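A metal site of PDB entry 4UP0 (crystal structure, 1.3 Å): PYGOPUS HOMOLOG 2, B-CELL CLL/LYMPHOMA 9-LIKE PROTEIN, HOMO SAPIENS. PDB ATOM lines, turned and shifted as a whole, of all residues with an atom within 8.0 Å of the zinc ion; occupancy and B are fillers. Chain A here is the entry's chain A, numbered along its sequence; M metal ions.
The side-chain hydroxyl (OG) of Ser 24 lies close to the side-chain sulfur (SG) of Cys 57 (3.0 Å). The side-chain sulfur (SG) of Cys 25 sits close to the backbone NH (N) of Lys 27, at 3.7 Å. O of Cys 21 is in hydrogen-bond range of N of Gln 26 (2.8 Å). The backbone NH (N) of Cys 21 sits at hydrogen-bond distance from the backbone carbonyl oxygen (O) of Lys 27 (2.9 Å). The backbone NH (N) of Leu 56 lies close to the side-chain sulfur (SG) of Cys 54 (3.4 Å).
The nearest printed residue that does not touch the zinc ion is Ser 24 (4.4 Å).
The zinc ion is bound by SG of Cys 54 (2.3 Å), SG of Cys 25 (2.3 Å), SG of Cys 57 (2.3 Å) and SG of Cys 21 (2.4 Å). The zinc ion has four donor atoms within binding distance.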
ATOM      1  N   GLY A   6      32.253  11.896 -14.698  1.00  0.00           N
ATOM      2  CA  GLY A   6      31.307  11.520 -13.634  1.00  0.00           C
ATOM      3  C   GLY A   6      31.213  10.002 -13.398  1.00  0.00           C
ATOM      4  O   GLY A   6      30.748   9.563 -12.350  1.00  0.00           O
ATOM      5  N   LEU A  20      27.931  16.385 -21.524  1.00  0.00           N
ATOM      6  CA  LEU A  20      27.572  17.024 -20.238  1.00  0.00           C
ATOM      7  C   LEU A  20      26.170  16.570 -19.843  1.00  0.00           C
ATOM      8  O   LEU A  20      25.191  16.584 -20.633  1.00  0.00           O
ATOM      9  CB  LEU A  20      27.572  18.532 -20.504  1.00  0.00           C
ATOM     10  CG  LEU A  20      27.175  19.414 -19.290  1.00  0.00           C
ATOM     11  CD1 LEU A  20      28.190  19.233 -18.192  1.00  0.00           C
ATOM     12  CD2 LEU A  20      27.182  20.878 -19.747  1.00  0.00           C
ATOM     13  N   CYS A  21      26.010  16.171 -18.572  1.00  0.00           N
ATOM     14  CA  CYS A  21      24.637  15.840 -18.051  1.00  0.00           C
ATOM     15  C   CYS A  21      23.878  17.153 -17.750  1.00  0.00           C
ATOM     16  O   CYS A  21      23.904  17.705 -16.660  1.00  0.00           O
ATOM     17  CB  CYS A  21      24.802  14.950 -16.824  1.00  0.00           C
ATOM     18  SG  CYS A  21      23.165  14.550 -16.090  1.00  0.00           S
ATOM     19  N   GLU A  22      23.305  17.706 -18.788  1.00  0.00           N
ATOM     20  CA  GLU A  22      22.608  18.955 -18.635  1.00  0.00           C
ATOM     21  C   GLU A  22      21.226  18.701 -17.973  1.00  0.00           C
ATOM     22  O   GLU A  22      20.557  19.617 -17.479  1.00  0.00           O
ATOM     23  CB  GLU A  22      22.374  19.640 -19.979  1.00  0.00           C
ATOM     24  CG  GLU A  22      23.664  20.137 -20.571  1.00  0.00           C
ATOM     25  CD  GLU A  22      23.436  20.773 -21.893  1.00  0.00           C
ATOM     26  OE1 GLU A  22      23.180  20.016 -22.855  1.00  0.00           O
ATOM     27  OE2 GLU A  22      23.525  22.024 -22.006  1.00  0.00           O
ATOM     28  N   ALA A  23      20.744  17.477 -18.040  1.00  0.00           N
ATOM     29  CA  ALA A  23      19.422  17.238 -17.473  1.00  0.00           C
ATOM     30  C   ALA A  23      19.489  17.468 -15.945  1.00  0.00           C
ATOM     31  O   ALA A  23      18.469  17.742 -15.343  1.00  0.00           O
ATOM     32  CB  ALA A  23      18.952  15.865 -17.831  1.00  0.00           C
ATOM     33  N   SER A  24      20.633  17.337 -15.307  1.00  0.00           N
ATOM     34  CA  SER A  24      20.644  17.248 -13.878  1.00  0.00           C
ATOM     35  C   SER A  24      21.992  17.670 -13.214  1.00  0.00           C
ATOM     36  O   SER A  24      22.144  18.789 -12.715  1.00  0.00           O
ATOM     37  CB  SER A  24      20.259  15.824 -13.533  1.00  0.00           C
ATOM     38  OG  SER A  24      20.363  15.610 -12.145  1.00  0.00           O
ATOM     39  N   CYS A  25      23.019  16.830 -13.290  1.00  0.00           N
ATOM     40  CA  CYS A  25      24.161  17.059 -12.365  1.00  0.00           C
ATOM     41  C   CYS A  25      25.226  17.944 -12.958  1.00  0.00           C
ATOM     42  O   CYS A  25      26.099  18.373 -12.190  1.00  0.00           O
ATOM     43  CB  CYS A  25      24.722  15.685 -11.939  1.00  0.00           C
ATOM     44  SG  CYS A  25      25.581  14.723 -13.263  1.00  0.00           S
ATOM     45  N   GLN A  26      25.219  18.225 -14.255  1.00  0.00           N
ATOM     46  CA  GLN A  26      26.199  19.126 -14.870  1.00  0.00           C
ATOM     47  C   GLN A  26      27.625  18.627 -14.738  1.00  0.00           C
ATOM     48  O   GLN A  26      28.570  19.417 -14.791  1.00  0.00           O
ATOM     49  CB  GLN A  26      26.071  20.556 -14.362  1.00  0.00           C
ATOM     50  CG  GLN A  26      24.643  21.008 -14.148  1.00  0.00           C
ATOM     51  CD  GLN A  26      23.911  21.036 -15.432  1.00  0.00           C
ATOM     52  OE1 GLN A  26      24.489  21.409 -16.484  1.00  0.00           O
ATOM     53  NE2 GLN A  26      22.572  20.781 -15.365  1.00  0.00           N
ATOM     54  N   LYS A  27      27.802  17.309 -14.712  1.00  0.00           N
ATOM     55  CA  LYS A  27      29.115  16.712 -14.780  1.00  0.00           C
ATOM     56  C   LYS A  27      29.354  16.244 -16.234  1.00  0.00           C
ATOM     57  O   LYS A  27      28.396  15.868 -16.943  1.00  0.00           O
ATOM     58  CB  LYS A  27      29.238  15.481 -13.850  1.00  0.00           C
ATOM     59  CG  LYS A  27      29.096  15.836 -12.359  1.00  0.00           C
ATOM     60  CD  LYS A  27      29.167  14.590 -11.539  1.00  0.00           C
ATOM     61  CE  LYS A  27      29.091  14.899 -10.032  1.00  0.00           C
ATOM     62  NZ  LYS A  27      29.015  13.630  -9.236  1.00  0.00           N
ATOM     63  N   TRP A  28      30.597  16.267 -16.672  1.00  0.00           N
ATOM     64  CA  TRP A  28      31.023  15.706 -17.934  1.00  0.00           C
ATOM     65  C   TRP A  28      31.292  14.203 -17.813  1.00  0.00           C
ATOM     66  O   TRP A  28      31.822  13.778 -16.775  1.00  0.00           O
ATOM     67  CB  TRP A  28      32.326  16.384 -18.393  1.00  0.00           C
ATOM     68  CG  TRP A  28      32.076  17.768 -18.907  1.00  0.00           C
ATOM     69  CD1 TRP A  28      32.136  18.983 -18.201  1.00  0.00           C
ATOM     70  CD2 TRP A  28      31.683  18.121 -20.232  1.00  0.00           C
ATOM     71  NE1 TRP A  28      31.796  20.015 -19.065  1.00  0.00           N
ATOM     72  CE2 TRP A  28      31.497  19.520 -20.300  1.00  0.00           C
ATOM     73  CE3 TRP A  28      31.462  17.350 -21.388  1.00  0.00           C
ATOM     74  CZ2 TRP A  28      31.116  20.152 -21.472  1.00  0.00           C
ATOM     75  CZ3 TRP A  28      31.084  17.984 -22.547  1.00  0.00           C
ATOM     76  CH2 TRP A  28      30.935  19.394 -22.596  1.00  0.00           C
ATOM     77  N   PHE A  29      30.964  13.459 -18.879  1.00  0.00           N
ATOM     78  CA  PHE A  29      31.229  12.037 -18.933  1.00  0.00           C
ATOM     79  C   PHE A  29      31.910  11.685 -20.243  1.00  0.00           C
ATOM     80  O   PHE A  29      31.427  12.074 -21.299  1.00  0.00           O
ATOM     81  CB  PHE A  29      29.901  11.267 -18.900  1.00  0.00           C
ATOM     82  CG  PHE A  29      29.220  11.257 -17.547  1.00  0.00           C
ATOM     83  CD1 PHE A  29      28.595  12.419 -17.034  1.00  0.00           C
ATOM     84  CD2 PHE A  29      29.214  10.085 -16.791  1.00  0.00           C
ATOM     85  CE1 PHE A  29      27.948  12.362 -15.797  1.00  0.00           C
ATOM     86  CE2 PHE A  29      28.574  10.032 -15.527  1.00  0.00           C
ATOM     87  CZ  PHE A  29      28.005  11.174 -15.044  1.00  0.00           C
ATOM     88  N   TRP A  52      21.014  15.517 -22.391  1.00  0.00           N
ATOM     89  CA  TRP A  52      21.326  14.160 -21.938  1.00  0.00           C
ATOM     90  C   TRP A  52      21.312  14.091 -20.390  1.00  0.00           C
ATOM     91  O   TRP A  52      21.711  15.028 -19.718  1.00  0.00           O
ATOM     92  CB  TRP A  52      22.715  13.786 -22.473  1.00  0.00           C
ATOM     93  CG  TRP A  52      23.187  12.433 -22.077  1.00  0.00           C
ATOM     94  CD1 TRP A  52      22.736  11.214 -22.496  1.00  0.00           C
ATOM     95  CD2 TRP A  52      24.242  12.198 -21.131  1.00  0.00           C
ATOM     96  NE1 TRP A  52      23.467  10.214 -21.858  1.00  0.00           N
ATOM     97  CE2 TRP A  52      24.407  10.801 -21.044  1.00  0.00           C
ATOM     98  CE3 TRP A  52      25.032  13.025 -20.344  1.00  0.00           C
ATOM     99  CZ2 TRP A  52      25.346  10.219 -20.209  1.00  0.00           C
ATOM    100  CZ3 TRP A  52      25.981  12.450 -19.542  1.00  0.00           C
ATOM    101  CH2 TRP A  52      26.164  11.049 -19.487  1.00  0.00           C
ATOM    102  N   ALA A  53      20.851  12.941 -19.896  1.00  0.00           N
ATOM    103  CA  ALA A  53      20.845  12.636 -18.460  1.00  0.00           C
ATOM    104  C   ALA A  53      21.721  11.379 -18.260  1.00  0.00           C
ATOM    105  O   ALA A  53      21.521  10.352 -18.964  1.00  0.00           O
ATOM    106  CB  ALA A  53      19.400  12.336 -18.048  1.00  0.00           C
ATOM    107  N   CYS A  54      22.704  11.487 -17.383  1.00  0.00           N
ATOM    108  CA  CYS A  54      23.570  10.366 -17.103  1.00  0.00           C
ATOM    109  C   CYS A  54      22.854   9.244 -16.311  1.00  0.00           C
ATOM    110  O   CYS A  54      21.698   9.403 -15.829  1.00  0.00           O
ATOM    111  CB  CYS A  54      24.789  10.819 -16.257  1.00  0.00           C
ATOM    112  SG  CYS A  54      24.426  11.192 -14.504  1.00  0.00           S
ATOM    113  N   ASP A  55      23.525   8.134 -16.125  1.00  0.00           N
ATOM    114  CA  ASP A  55      23.017   6.918 -15.418  1.00  0.00           C
ATOM    115  C   ASP A  55      22.816   7.131 -13.955  1.00  0.00           C
ATOM    116  O   ASP A  55      22.025   6.426 -13.341  1.00  0.00           O
ATOM    117  CB  ASP A  55      24.038   5.769 -15.656  1.00  0.00           C
ATOM    118  CG  ASP A  55      23.536   4.418 -15.227  1.00  0.00           C
ATOM    119  OD1 ASP A  55      22.567   3.973 -15.855  1.00  0.00           O
ATOM    120  OD2 ASP A  55      24.111   3.768 -14.282  1.00  0.00           O
ATOM    121  N   LEU A  56      23.554   8.082 -13.393  1.00  0.00           N
ATOM    122  CA  LEU A  56      23.417   8.405 -11.956  1.00  0.00           C
ATOM    123  C   LEU A  56      22.213   9.240 -11.653  1.00  0.00           C
ATOM    124  O   LEU A  56      21.685   9.188 -10.551  1.00  0.00           O
ATOM    125  CB  LEU A  56      24.653   9.102 -11.400  1.00  0.00           C
ATOM    126  CG  LEU A  56      26.066   8.652 -11.802  1.00  0.00           C
ATOM    127  CD1 LEU A  56      27.109   9.533 -11.143  1.00  0.00           C
ATOM    128  CD2 LEU A  56      26.356   7.203 -11.504  1.00  0.00           C
ATOM    129  N   CYS A  57      21.763  10.029 -12.612  1.00  0.00           N
ATOM    130  CA  CYS A  57      20.675  10.976 -12.404  1.00  0.00           C
ATOM    131  C   CYS A  57      19.301  10.384 -12.723  1.00  0.00           C
ATOM    132  O   CYS A  57      19.016  10.140 -13.897  1.00  0.00           O
ATOM    133  CB  CYS A  57      20.950  12.288 -13.205  1.00  0.00           C
ATOM    134  SG  CYS A  57      22.273  13.277 -12.477  1.00  0.00           S
HETATM  135 ZN    ZN M   1      23.881  13.419 -14.156  1.00  0.00          ZN
